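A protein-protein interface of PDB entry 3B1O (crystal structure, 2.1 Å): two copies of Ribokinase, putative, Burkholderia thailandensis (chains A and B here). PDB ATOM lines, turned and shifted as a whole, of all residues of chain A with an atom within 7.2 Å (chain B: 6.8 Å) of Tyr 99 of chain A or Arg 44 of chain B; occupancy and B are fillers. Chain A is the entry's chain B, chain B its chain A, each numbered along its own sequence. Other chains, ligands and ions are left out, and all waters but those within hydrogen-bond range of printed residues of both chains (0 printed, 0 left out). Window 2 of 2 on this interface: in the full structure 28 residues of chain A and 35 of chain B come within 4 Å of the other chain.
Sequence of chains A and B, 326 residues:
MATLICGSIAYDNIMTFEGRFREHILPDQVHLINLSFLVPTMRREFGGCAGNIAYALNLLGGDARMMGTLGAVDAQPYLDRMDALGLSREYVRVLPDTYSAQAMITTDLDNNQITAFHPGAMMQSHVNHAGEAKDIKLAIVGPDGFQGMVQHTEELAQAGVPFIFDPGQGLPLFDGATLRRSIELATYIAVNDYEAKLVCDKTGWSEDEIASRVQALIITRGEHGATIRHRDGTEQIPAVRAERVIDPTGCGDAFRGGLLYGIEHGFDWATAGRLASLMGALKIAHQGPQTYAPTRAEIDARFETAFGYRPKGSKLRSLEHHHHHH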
ATOM      1  N   TYR A  11     -13.339   2.340  17.729  1.00  0.00           N
ATOM      2  CA  TYR A  11     -12.487   3.487  17.962  1.00  0.00           C
ATOM      3  C   TYR A  11     -11.270   3.044  18.746  1.00  0.00           C
ATOM      4  O   TYR A  11     -11.360   2.185  19.619  1.00  0.00           O
ATOM      5  CB  TYR A  11     -13.205   4.555  18.800  1.00  0.00           C
ATOM      6  CG  TYR A  11     -14.392   5.224  18.149  1.00  0.00           C
ATOM      7  CD1 TYR A  11     -14.220   6.176  17.147  1.00  0.00           C
ATOM      8  CD2 TYR A  11     -15.687   4.930  18.563  1.00  0.00           C
ATOM      9  CE1 TYR A  11     -15.310   6.803  16.557  1.00  0.00           C
ATOM     10  CE2 TYR A  11     -16.783   5.536  17.978  1.00  0.00           C
ATOM     11  CZ  TYR A  11     -16.592   6.477  16.979  1.00  0.00           C
ATOM     12  OH  TYR A  11     -17.683   7.099  16.407  1.00  0.00           O
ATOM     13  N   THR A  69     -22.110  -2.379  13.963  1.00  0.00           N
ATOM     14  CA  THR A  69     -22.887  -1.650  14.962  1.00  0.00           C
ATOM     15  C   THR A  69     -22.001  -0.678  15.746  1.00  0.00           C
ATOM     16  O   THR A  69     -20.881  -1.021  16.154  1.00  0.00           O
ATOM     17  CB  THR A  69     -23.638  -2.614  15.912  1.00  0.00           C
ATOM     18  OG1 THR A  69     -22.810  -3.751  16.176  1.00  0.00           O
ATOM     19  CG2 THR A  69     -24.949  -3.092  15.279  1.00  0.00           C
ATOM     20  N   LEU A  70     -22.494   0.545  15.902  1.00  0.00           N
ATOM     21  CA  LEU A  70     -21.836   1.545  16.723  1.00  0.00           C
ATOM     22  C   LEU A  70     -22.704   1.754  17.950  1.00  0.00           C
ATOM     23  O   LEU A  70     -23.805   1.198  18.029  1.00  0.00           O
ATOM     24  CB  LEU A  70     -21.643   2.853  15.938  1.00  0.00           C
ATOM     25  CG  LEU A  70     -20.455   2.956  14.963  1.00  0.00           C
ATOM     26  CD1 LEU A  70     -20.723   3.935  13.835  1.00  0.00           C
ATOM     27  CD2 LEU A  70     -19.137   3.311  15.675  1.00  0.00           C
ATOM     28  N   GLY A  71     -22.202   2.521  18.916  1.00  0.00           N
ATOM     29  CA  GLY A  71     -22.979   2.902  20.095  1.00  0.00           C
ATOM     30  C   GLY A  71     -23.458   4.343  20.009  1.00  0.00           C
ATOM     31  O   GLY A  71     -22.702   5.224  19.614  1.00  0.00           O
ATOM     32  N   ALA A  72     -24.715   4.576  20.390  1.00  0.00           N
ATOM     33  CA  ALA A  72     -25.322   5.916  20.376  1.00  0.00           C
ATOM     34  C   ALA A  72     -24.588   6.920  21.254  1.00  0.00           C
ATOM     35  O   ALA A  72     -24.618   8.127  20.995  1.00  0.00           O
ATOM     36  CB  ALA A  72     -26.804   5.845  20.773  1.00  0.00           C
ATOM     37  N   VAL A  73     -23.932   6.420  22.297  1.00  0.00           N
ATOM     38  CA  VAL A  73     -23.147   7.284  23.162  1.00  0.00           C
ATOM     39  C   VAL A  73     -22.047   7.971  22.338  1.00  0.00           C
ATOM     40  O   VAL A  73     -21.848   9.184  22.466  1.00  0.00           O
ATOM     41  CB  VAL A  73     -22.567   6.514  24.362  1.00  0.00           C
ATOM     42  CG1 VAL A  73     -21.483   7.336  25.052  1.00  0.00           C
ATOM     43  CG2 VAL A  73     -23.687   6.131  25.354  1.00  0.00           C
ATOM     44  N   ASP A  74     -21.372   7.210  21.470  1.00  0.00           N
ATOM     45  CA  ASP A  74     -20.226   7.747  20.715  1.00  0.00           C
ATOM     46  C   ASP A  74     -20.165   7.360  19.220  1.00  0.00           C
ATOM     47  O   ASP A  74     -19.103   7.025  18.698  1.00  0.00           O
ATOM     48  CB  ASP A  74     -18.895   7.416  21.433  1.00  0.00           C
ATOM     49  CG  ASP A  74     -18.829   5.968  21.942  1.00  0.00           C
ATOM     50  OD1 ASP A  74     -19.463   5.083  21.335  1.00  0.00           O
ATOM     51  OD2 ASP A  74     -18.139   5.716  22.955  1.00  0.00           O
ATOM     52  N   ALA A  75     -21.291   7.445  18.525  1.00  0.00           N
ATOM     53  CA  ALA A  75     -21.324   7.067  17.107  1.00  0.00           C
ATOM     54  C   ALA A  75     -20.938   8.219  16.170  1.00  0.00           C
ATOM     55  O   ALA A  75     -20.319   7.996  15.130  1.00  0.00           O
ATOM     56  CB  ALA A  75     -22.694   6.506  16.735  1.00  0.00           C
ATOM     57  N   LEU A  95     -26.964   1.670  18.172  1.00  0.00           N
ATOM     58  CA  LEU A  95     -27.767   1.098  19.259  1.00  0.00           C
ATOM     59  C   LEU A  95     -27.782   2.027  20.472  1.00  0.00           C
ATOM     60  O   LEU A  95     -26.741   2.584  20.838  1.00  0.00           O
ATOM     61  CB  LEU A  95     -27.213  -0.269  19.681  1.00  0.00           C
ATOM     62  CG  LEU A  95     -26.848  -1.313  18.615  1.00  0.00           C
ATOM     63  CD1 LEU A  95     -25.828  -2.284  19.185  1.00  0.00           C
ATOM     64  CD2 LEU A  95     -28.080  -2.048  18.089  1.00  0.00           C
ATOM     65  N   PRO A  96     -28.953   2.172  21.124  1.00  0.00           N
ATOM     66  CA  PRO A  96     -29.034   3.093  22.257  1.00  0.00           C
ATOM     67  C   PRO A  96     -28.403   2.517  23.522  1.00  0.00           C
ATOM     68  O   PRO A  96     -28.282   1.293  23.649  1.00  0.00           O
ATOM     69  CB  PRO A  96     -30.552   3.279  22.464  1.00  0.00           C
ATOM     70  CG  PRO A  96     -31.234   2.371  21.477  1.00  0.00           C
ATOM     71  CD  PRO A  96     -30.209   1.422  20.944  1.00  0.00           C
ATOM     72  N   ASP A  97     -28.011   3.412  24.431  1.00  0.00           N
ATOM     73  CA  ASP A  97     -27.477   3.085  25.769  1.00  0.00           C
ATOM     74  C   ASP A  97     -26.302   2.088  25.758  1.00  0.00           C
ATOM     75  O   ASP A  97     -26.146   1.251  26.656  1.00  0.00           O
ATOM     76  CB  ASP A  97     -28.610   2.725  26.770  1.00  0.00           C
ATOM     77  CG  ASP A  97     -28.945   1.236  26.809  1.00  0.00           C
ATOM     78  OD1 ASP A  97     -29.459   0.678  25.811  1.00  0.00           O
ATOM     79  OD2 ASP A  97     -28.720   0.625  27.877  1.00  0.00           O
ATOM     80  N   THR A  98     -25.489   2.191  24.708  1.00  0.00           N
ATOM     81  CA  THR A  98     -24.280   1.391  24.560  1.00  0.00           C
ATOM     82  C   THR A  98     -23.156   2.269  24.025  1.00  0.00           C
ATOM     83  O   THR A  98     -23.400   3.295  23.360  1.00  0.00           O
ATOM     84  CB  THR A  98     -24.452   0.155  23.600  1.00  0.00           C
ATOM     85  OG1 THR A  98     -24.289   0.557  22.231  1.00  0.00           O
ATOM     86  CG2 THR A  98     -25.807  -0.553  23.796  1.00  0.00           C
ATOM     87  N   TYR A  99     -21.932   1.861  24.343  1.00  0.00           N
ATOM     88  CA  TYR A  99     -20.748   2.474  23.809  1.00  0.00           C
ATOM     89  C   TYR A  99     -20.326   1.687  22.569  1.00  0.00           C
ATOM     90  O   TYR A  99     -20.523   0.483  22.486  1.00  0.00           O
ATOM     91  CB  TYR A  99     -19.623   2.419  24.849  1.00  0.00           C
ATOM     92  CG  TYR A  99     -19.802   3.296  26.088  1.00  0.00           C
ATOM     93  CD1 TYR A  99     -19.233   4.567  26.148  1.00  0.00           C
ATOM     94  CD2 TYR A  99     -20.509   2.838  27.209  1.00  0.00           C
ATOM     95  CE1 TYR A  99     -19.374   5.365  27.281  1.00  0.00           C
ATOM     96  CE2 TYR A  99     -20.659   3.631  28.339  1.00  0.00           C
ATOM     97  CZ  TYR A  99     -20.082   4.886  28.369  1.00  0.00           C
ATOM     98  OH  TYR A  99     -20.210   5.673  29.485  1.00  0.00           O
ATOM     99  N   SER A 100     -19.734   2.384  21.610  1.00  0.00           N
ATOM    100  CA  SER A 100     -19.111   1.734  20.476  1.00  0.00           C
ATOM    101  C   SER A 100     -17.922   0.906  20.957  1.00  0.00           C
ATOM    102  O   SER A 100     -17.298   1.227  21.982  1.00  0.00           O
ATOM    103  CB  SER A 100     -18.635   2.781  19.470  1.00  0.00           C
ATOM    104  OG  SER A 100     -19.686   3.657  19.096  1.00  0.00           O
ATOM    105  N   ALA A 101     -17.640  -0.180  20.235  1.00  0.00           N
ATOM    106  CA  ALA A 101     -16.419  -0.949  20.426  1.00  0.00           C
ATOM    107  C   ALA A 101     -15.264   0.009  20.422  1.00  0.00           C
ATOM    108  O   ALA A 101     -15.147   0.849  19.509  1.00  0.00           O
ATOM    109  CB  ALA A 101     -16.236  -1.960  19.300  1.00  0.00           C
ATOM    110  N   GLN A 102     -14.415  -0.116  21.444  1.00  0.00           N
ATOM    111  CA  GLN A 102     -13.272   0.772  21.604  1.00  0.00           C
ATOM    112  C   GLN A 102     -12.207   0.242  22.555  1.00  0.00           C
ATOM    113  O   GLN A 102     -12.497  -0.450  23.537  1.00  0.00           O
ATOM    114  CB  GLN A 102     -13.716   2.167  22.064  1.00  0.00           C
ATOM    115  CG  GLN A 102     -14.592   2.158  23.297  1.00  0.00           C
ATOM    116  CD  GLN A 102     -15.325   3.473  23.484  1.00  0.00           C
ATOM    117  OE1 GLN A 102     -14.708   4.519  23.700  1.00  0.00           O
ATOM    118  NE2 GLN A 102     -16.649   3.426  23.402  1.00  0.00           N
ATOM    119  N   HIS A 118     -13.142  -2.411  25.546  1.00  0.00           N
ATOM    120  CA  HIS A 118     -14.557  -2.603  25.793  1.00  0.00           C
ATOM    121  C   HIS A 118     -15.211  -3.012  24.477  1.00  0.00           C
ATOM    122  O   HIS A 118     -15.250  -2.216  23.533  1.00  0.00           O
ATOM    123  CB  HIS A 118     -15.194  -1.319  26.310  1.00  0.00           C
ATOM    124  CG  HIS A 118     -16.663  -1.435  26.565  1.00  0.00           C
ATOM    125  ND1 HIS A 118     -17.179  -2.186  27.598  1.00  0.00           N
ATOM    126  CD2 HIS A 118     -17.728  -0.888  25.930  1.00  0.00           C
ATOM    127  CE1 HIS A 118     -18.498  -2.107  27.583  1.00  0.00           C
ATOM    128  NE2 HIS A 118     -18.855  -1.322  26.584  1.00  0.00           N
ATOM    129  N   PRO A 119     -15.701  -4.259  24.406  1.00  0.00           N
ATOM    130  CA  PRO A 119     -16.370  -4.814  23.214  1.00  0.00           C
ATOM    131  C   PRO A 119     -17.571  -3.958  22.750  1.00  0.00           C
ATOM    132  O   PRO A 119     -17.669  -3.619  21.562  1.00  0.00           O
ATOM    133  CB  PRO A 119     -16.818  -6.197  23.690  1.00  0.00           C
ATOM    134  CG  PRO A 119     -15.854  -6.544  24.803  1.00  0.00           C
ATOM    135  CD  PRO A 119     -15.606  -5.250  25.497  1.00  0.00           C
ATOM    136  N   GLY A 120     -18.452  -3.600  23.687  1.00  0.00           N
ATOM    137  CA  GLY A 120     -19.540  -2.657  23.418  1.00  0.00           C
ATOM    138  C   GLY A 120     -20.471  -3.104  22.312  1.00  0.00           C
ATOM    139  O   GLY A 120     -20.815  -4.287  22.220  1.00  0.00           O
ATOM    140  N   ALA A 121     -20.847  -2.155  21.452  1.00  0.00           N
ATOM    141  CA  ALA A 121     -21.831  -2.359  20.372  1.00  0.00           C
ATOM    142  C   ALA A 121     -21.546  -3.540  19.437  1.00  0.00           C
ATOM    143  O   ALA A 121     -22.448  -4.036  18.756  1.00  0.00           O
ATOM    144  CB  ALA A 121     -21.984  -1.089  19.571  1.00  0.00           C
ATOM    145  N   MET A 122     -20.291  -3.981  19.411  1.00  0.00           N
ATOM    146  CA  MET A 122     -19.847  -5.092  18.577  1.00  0.00           C
ATOM    147  C   MET A 122     -20.478  -6.414  19.026  1.00  0.00           C
ATOM    148  O   MET A 122     -20.724  -7.304  18.198  1.00  0.00           O
ATOM    149  CB  MET A 122     -18.319  -5.177  18.619  1.00  0.00           C
ATOM    150  CG  MET A 122     -17.709  -6.349  17.870  1.00  0.00           C
ATOM    151  SD  MET A 122     -16.019  -6.636  18.410  1.00  0.00           S
ATOM    152  CE  MET A 122     -16.268  -7.328  20.044  1.00  0.00           C
ATOM    153  N   TYR B  11     -19.484  14.018  32.218  1.00  0.00           N
ATOM    154  CA  TYR B  11     -20.053  12.688  32.109  1.00  0.00           C
ATOM    155  C   TYR B  11     -18.964  11.710  32.523  1.00  0.00           C
ATOM    156  O   TYR B  11     -17.836  11.760  32.009  1.00  0.00           O
ATOM    157  CB  TYR B  11     -20.538  12.414  30.688  1.00  0.00           C
ATOM    158  CG  TYR B  11     -21.696  13.296  30.274  1.00  0.00           C
ATOM    159  CD1 TYR B  11     -23.004  12.979  30.638  1.00  0.00           C
ATOM    160  CD2 TYR B  11     -21.483  14.449  29.504  1.00  0.00           C
ATOM    161  CE1 TYR B  11     -24.059  13.786  30.255  1.00  0.00           C
ATOM    162  CE2 TYR B  11     -22.519  15.262  29.136  1.00  0.00           C
ATOM    163  CZ  TYR B  11     -23.807  14.928  29.511  1.00  0.00           C
ATOM    164  OH  TYR B  11     -24.847  15.734  29.128  1.00  0.00           O
ATOM    165  N   ASP B  12     -19.284  10.856  33.488  1.00  0.00           N
ATOM    166  CA  ASP B  12     -18.348   9.841  33.930  1.00  0.00           C
ATOM    167  C   ASP B  12     -18.589   8.582  33.111  1.00  0.00           C
ATOM    168  O   ASP B  12     -19.729   8.178  32.888  1.00  0.00           O
ATOM    169  CB  ASP B  12     -18.480   9.574  35.429  1.00  0.00           C
ATOM    170  CG  ASP B  12     -17.927  10.720  36.296  1.00  0.00           C
ATOM    171  OD1 ASP B  12     -18.153  10.700  37.525  1.00  0.00           O
ATOM    172  OD2 ASP B  12     -17.252  11.631  35.768  1.00  0.00           O
ATOM    173  N   ASN B  13     -17.497   8.010  32.619  1.00  0.00           N
ATOM    174  CA  ASN B  13     -17.519   6.745  31.928  1.00  0.00           C
ATOM    175  C   ASN B  13     -16.743   5.763  32.784  1.00  0.00           C
ATOM    176  O   ASN B  13     -15.510   5.746  32.781  1.00  0.00           O
ATOM    177  CB  ASN B  13     -16.932   6.895  30.532  1.00  0.00           C
ATOM    178  CG  ASN B  13     -17.620   7.983  29.731  1.00  0.00           C
ATOM    179  OD1 ASN B  13     -18.702   7.778  29.219  1.00  0.00           O
ATOM    180  ND2 ASN B  13     -16.990   9.159  29.632  1.00  0.00           N
ATOM    181  N   ILE B  14     -17.487   4.977  33.551  1.00  0.00           N
ATOM    182  CA  ILE B  14     -16.920   4.163  34.618  1.00  0.00           C
ATOM    183  C   ILE B  14     -16.746   2.728  34.142  1.00  0.00           C
ATOM    184  O   ILE B  14     -17.695   2.092  33.675  1.00  0.00           O
ATOM    185  CB  ILE B  14     -17.778   4.252  35.921  1.00  0.00           C
ATOM    186  CG1 ILE B  14     -17.921   5.729  36.343  1.00  0.00           C
ATOM    187  CG2 ILE B  14     -17.160   3.411  37.040  1.00  0.00           C
ATOM    188  CD1 ILE B  14     -18.700   5.964  37.632  1.00  0.00           C
ATOM    189  N   THR B  41     -17.932  -4.031  31.021  1.00  0.00           N
ATOM    190  CA  THR B  41     -18.984  -3.069  31.318  1.00  0.00           C
ATOM    191  C   THR B  41     -18.448  -1.643  31.398  1.00  0.00           C
ATOM    192  O   THR B  41     -17.408  -1.391  32.013  1.00  0.00           O
ATOM    193  CB  THR B  41     -19.759  -3.412  32.634  1.00  0.00           C
ATOM    194  OG1 THR B  41     -19.179  -2.715  33.744  1.00  0.00           O
ATOM    195  CG2 THR B  41     -19.780  -4.927  32.918  1.00  0.00           C
ATOM    196  N   MET B  42     -19.168  -0.726  30.754  1.00  0.00           N
ATOM    197  CA  MET B  42     -18.934   0.701  30.881  1.00  0.00           C
ATOM    198  C   MET B  42     -20.249   1.339  31.336  1.00  0.00           C
ATOM    199  O   MET B  42     -21.278   1.121  30.705  1.00  0.00           O
ATOM    200  CB  MET B  42     -18.526   1.316  29.535  1.00  0.00           C
ATOM    201  CG  MET B  42     -17.138   0.988  29.017  1.00  0.00           C
ATOM    202  SD  MET B  42     -16.394   2.399  28.149  1.00  0.00           S
ATOM    203  CE  MET B  42     -16.553   1.923  26.449  1.00  0.00           C
ATOM    204  N   ARG B  43     -20.212   2.111  32.424  1.00  0.00           N
ATOM    205  CA  ARG B  43     -21.403   2.794  32.956  1.00  0.00           C
ATOM    206  C   ARG B  43     -21.292   4.304  32.770  1.00  0.00           C
ATOM    207  O   ARG B  43     -20.329   4.929  33.236  1.00  0.00           O
ATOM    208  CB  ARG B  43     -21.609   2.489  34.447  1.00  0.00           C
ATOM    209  CG  ARG B  43     -22.611   1.366  34.774  1.00  0.00           C
ATOM    210  CD  ARG B  43     -22.798   1.174  36.303  1.00  0.00           C
ATOM    211  NE  ARG B  43     -21.522   1.236  37.032  1.00  0.00           N
ATOM    212  CZ  ARG B  43     -20.670   0.218  37.188  1.00  0.00           C
ATOM    213  NH1 ARG B  43     -20.942  -0.985  36.687  1.00  0.00           N
ATOM    214  NH2 ARG B  43     -19.527   0.403  37.852  1.00  0.00           N
ATOM    215  N   ARG B  44     -22.275   4.874  32.088  1.00  0.00           N
ATOM    216  CA  ARG B  44     -22.341   6.293  31.860  1.00  0.00           C
ATOM    217  C   ARG B  44     -23.099   6.963  33.006  1.00  0.00           C
ATOM    218  O   ARG B  44     -24.230   6.597  33.309  1.00  0.00           O
ATOM    219  CB  ARG B  44     -23.041   6.581  30.536  1.00  0.00           C
ATOM    220  CG  ARG B  44     -23.189   8.073  30.232  1.00  0.00           C
ATOM    221  CD  ARG B  44     -21.991   8.639  29.477  1.00  0.00           C
ATOM    222  NE  ARG B  44     -22.417   9.769  28.643  1.00  0.00           N
ATOM    223  CZ  ARG B  44     -21.616  10.471  27.846  1.00  0.00           C
ATOM    224  NH1 ARG B  44     -20.320  10.174  27.762  1.00  0.00           N
ATOM    225  NH2 ARG B  44     -22.117  11.479  27.133  1.00  0.00           N
ATOM    226  N   GLU B  45     -22.466   7.940  33.636  1.00  0.00           N
ATOM    227  CA  GLU B  45     -23.058   8.609  34.790  1.00  0.00           C
ATOM    228  C   GLU B  45     -22.844  10.120  34.776  1.00  0.00           C
ATOM    229  O   GLU B  45     -21.813  10.611  34.321  1.00  0.00           O
ATOM    230  CB  GLU B  45     -22.483   8.024  36.094  1.00  0.00           C
ATOM    231  CG  GLU B  45     -22.530   6.490  36.228  1.00  0.00           C
ATOM    232  CD  GLU B  45     -23.891   5.945  36.657  1.00  0.00           C
ATOM    233  OE1 GLU B  45     -24.848   6.724  36.830  1.00  0.00           O
ATOM    234  OE2 GLU B  45     -24.009   4.715  36.820  1.00  0.00           O
ATOM    235  N   PHE B  46     -23.818  10.856  35.302  1.00  0.00           N
ATOM    236  CA  PHE B  46     -23.655  12.288  35.567  1.00  0.00           C
ATOM    237  C   PHE B  46     -22.605  12.520  36.640  1.00  0.00           C
ATOM    238  O   PHE B  46     -22.704  11.969  37.738  1.00  0.00           O
ATOM    239  CB  PHE B  46     -24.994  12.866  36.005  1.00  0.00           C
ATOM    240  CG  PHE B  46     -26.083  12.660  34.986  1.00  0.00           C
ATOM    241  CD1 PHE B  46     -27.020  11.644  35.138  1.00  0.00           C
ATOM    242  CD2 PHE B  46     -26.140  13.466  33.846  1.00  0.00           C
ATOM    243  CE1 PHE B  46     -28.035  11.457  34.182  1.00  0.00           C
ATOM    244  CE2 PHE B  46     -27.143  13.274  32.880  1.00  0.00           C
ATOM    245  CZ  PHE B  46     -28.078  12.274  33.050  1.00  0.00           C
ATOM    246  N   ASP B  74     -23.212  17.553  23.452  1.00  0.00           N
ATOM    247  CA  ASP B  74     -23.736  16.517  24.351  1.00  0.00           C
ATOM    248  C   ASP B  74     -24.257  17.027  25.692  1.00  0.00           C
ATOM    249  O   ASP B  74     -24.410  16.237  26.641  1.00  0.00           O
ATOM    250  CB  ASP B  74     -22.674  15.426  24.567  1.00  0.00           C
ATOM    251  CG  ASP B  74     -21.419  15.950  25.259  1.00  0.00           C
ATOM    252  OD1 ASP B  74     -21.392  17.140  25.639  1.00  0.00           O
ATOM    253  OD2 ASP B  74     -20.462  15.159  25.445  1.00  0.00           O
ATOM    254  N   PRO B  77     -28.648  15.979  28.003  1.00  0.00           N
ATOM    255  CA  PRO B  77     -29.153  15.175  29.121  1.00  0.00           C
ATOM    256  C   PRO B  77     -28.772  15.746  30.478  1.00  0.00           C
ATOM    257  O   PRO B  77     -29.546  15.620  31.423  1.00  0.00           O
ATOM    258  CB  PRO B  77     -28.500  13.813  28.897  1.00  0.00           C
ATOM    259  CG  PRO B  77     -28.222  13.784  27.406  1.00  0.00           C
ATOM    260  CD  PRO B  77     -27.761  15.178  27.136  1.00  0.00           C
ATOM    261  N   TYR B  99     -17.354  19.173  22.976  1.00  0.00           N
ATOM    262  CA  TYR B  99     -17.840  18.145  23.885  1.00  0.00           C
ATOM    263  C   TYR B  99     -17.725  18.564  25.334  1.00  0.00           C
ATOM    264  O   TYR B  99     -16.759  19.214  25.717  1.00  0.00           O
ATOM    265  CB  TYR B  99     -17.046  16.850  23.705  1.00  0.00           C
ATOM    266  CG  TYR B  99     -17.563  16.001  22.591  1.00  0.00           C
ATOM    267  CD1 TYR B  99     -18.649  15.147  22.799  1.00  0.00           C
ATOM    268  CD2 TYR B  99     -16.994  16.059  21.321  1.00  0.00           C
ATOM    269  CE1 TYR B  99     -19.135  14.354  21.788  1.00  0.00           C
ATOM    270  CE2 TYR B  99     -17.475  15.275  20.292  1.00  0.00           C
ATOM    271  CZ  TYR B  99     -18.545  14.424  20.536  1.00  0.00           C
ATOM    272  OH  TYR B  99     -19.048  13.637  19.530  1.00  0.00           O
ATOM    273  N   SER B 100     -18.712  18.158  26.130  1.00  0.00           N
ATOM    274  CA  SER B 100     -18.633  18.248  27.571  1.00  0.00           C
ATOM    275  C   SER B 100     -17.450  17.430  28.052  1.00  0.00           C
ATOM    276  O   SER B 100     -17.018  16.489  27.381  1.00  0.00           O
ATOM    277  CB  SER B 100     -19.897  17.677  28.211  1.00  0.00           C
ATOM    278  OG  SER B 100     -20.978  18.570  28.042  1.00  0.00           O
ATOM    279  N   ALA B 101     -16.969  17.763  29.240  1.00  0.00           N
ATOM    280  CA  ALA B 101     -15.886  17.014  29.853  1.00  0.00           C
ATOM    281  C   ALA B 101     -16.291  15.543  29.963  1.00  0.00           C
ATOM    282  O   ALA B 101     -17.465  15.235  30.174  1.00  0.00           O
ATOM    283  CB  ALA B 101     -15.559  17.588  31.227  1.00  0.00           C
ATOM    284  N   GLN B 102     -15.320  14.662  29.766  1.00  0.00           N
ATOM    285  CA  GLN B 102     -15.502  13.207  29.851  1.00  0.00           C
ATOM    286  C   GLN B 102     -14.418  12.628  30.746  1.00  0.00           C
ATOM    287  O   GLN B 102     -13.223  12.786  30.459  1.00  0.00           O
ATOM    288  CB  GLN B 102     -15.352  12.541  28.483  1.00  0.00           C
ATOM    289  CG  GLN B 102     -16.272  13.061  27.377  1.00  0.00           C
ATOM    290  CD  GLN B 102     -17.688  12.565  27.511  1.00  0.00           C
ATOM    291  OE1 GLN B 102     -17.931  11.398  27.842  1.00  0.00           O
ATOM    292  NE2 GLN B 102     -18.649  13.454  27.248  1.00  0.00           N
ATOM    293  N   MET B 104     -12.790   9.190  31.868  1.00  0.00           N
ATOM    294  CA  MET B 104     -12.620   7.740  31.622  1.00  0.00           C
ATOM    295  C   MET B 104     -12.065   7.076  32.878  1.00  0.00           C
ATOM    296  O   MET B 104     -10.839   7.001  33.065  1.00  0.00           O
ATOM    297  CB  MET B 104     -11.668   7.451  30.446  1.00  0.00           C
ATOM    298  CG  MET B 104     -11.839   8.318  29.203  1.00  0.00           C
ATOM    299  SD  MET B 104     -13.559   8.538  28.758  1.00  0.00           S
ATOM    300  CE  MET B 104     -13.980   6.841  28.293  1.00  0.00           C
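The side-chain amide oxygen (OD1) of Asn 13 of chain B sits at hydrogen-bond distance from the side-chain hydroxyl (OH) of Tyr 99 of chain A.
The backbone NH (N) of Arg 44 of chain B lies close to the side-chain hydroxyl (OH) of Tyr 99 of chain A, at 3.4 Å.
Of the 17 printed residues of chain B, 5 touch a printed residue of chain A.
Hydrophobic or aromatic side chains of chain B that line the printed part of chain A: Met 42.
Of the 21 printed residues of chain A, 3 touch a printed residue of chain B.
Hydrophobic or aromatic side chains of chain A within 4 Å of the printed part of chain B: Tyr 99 and His 118.
Among the printed residues, 7 pairs touch across the chains.
Among the printed residues, no Asp or Glu carboxylate lies within 4 Å of a Lys or Arg side-chain nitrogen of the other chain.
Positions printed for both chains: 11, 74, 99, 100, 101 and 102.
Of the 7 pairs that touch across the chains among the printed residues, none has its exchanged pair printed and touching as well.
The side-chain amide nitrogen (NE2) of Gln 102 of chain A sits at hydrogen-bond distance from the backbone carbonyl oxygen (O) of Ser 100 of chain A.
The side-chain amide nitrogen (ND2) of Asn 13 of chain B sits at hydrogen-bond distance from the side-chain amide oxygen (OE1) of Gln 102 of chain B, at 3.0 Å.
O of Tyr 99 of chain A is in hydrogen-bond range of N of Ala 121 of chain A (2.9 Å).
The guanidinium group of Arg 44 of chain B lies within hydrogen-bond range of the side-chain amide oxygen of Gln 102 of chain B, 2.7 Å away.
The side-chain amide oxygen (OD1) of Asn 13 of chain B sits at hydrogen-bond distance from the guanidinium group (NH1) of Arg 44 of chain B (3.2 Å).
The backbone carbonyl oxygen of Ile 14 of chain B lies within hydrogen-bond range of the backbone NH of Arg 43 of chain B, at 2.8 Å.
Printed residues of chain B within 4 Å of Tyr 99 of chain A: Asn 13 (2.6 Å), Met 42 (3.4 Å), Arg 43 (3.7 Å) and Arg 44 (3.2 Å).
Of the printed residues of chain B, His 118 of chain A touches Thr 41 (3.8 Å) and Met 42 (3.1 Å).
Of the printed residues of chain A, Met 42 of chain B touches Tyr 99 (3.4 Å), Gln 102 (3.4 Å) and His 118 (3.1 Å).
Of the printed residues of chain A, Asn 13 of chain B touches Tyr 99 (2.6 Å).
Of the printed residues of chain B, Gln 102 of chain A touches Met 42.
The nearest residue of chain A that does not touch Arg 44 of chain B is Val 73 of chain A (4.1 Å).
The nearest printed residue of chain B that does not touch His 118 of chain A is Arg 43 of chain B (6.6 Å).
Among the printed residues, merely in contact across the chains: Tyr 99 of chain A with Met 42 of chain B (3.4 Å), Tyr 99 of chain A with Arg 43 of chain B (3.7 Å), Gln 102 of chain A with Met 42 of chain B (3.4 Å), His 118 of chain A with Thr 41 of chain B (3.8 Å) and His 118 of chain A with Met 42 of chain B (3.1 Å).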
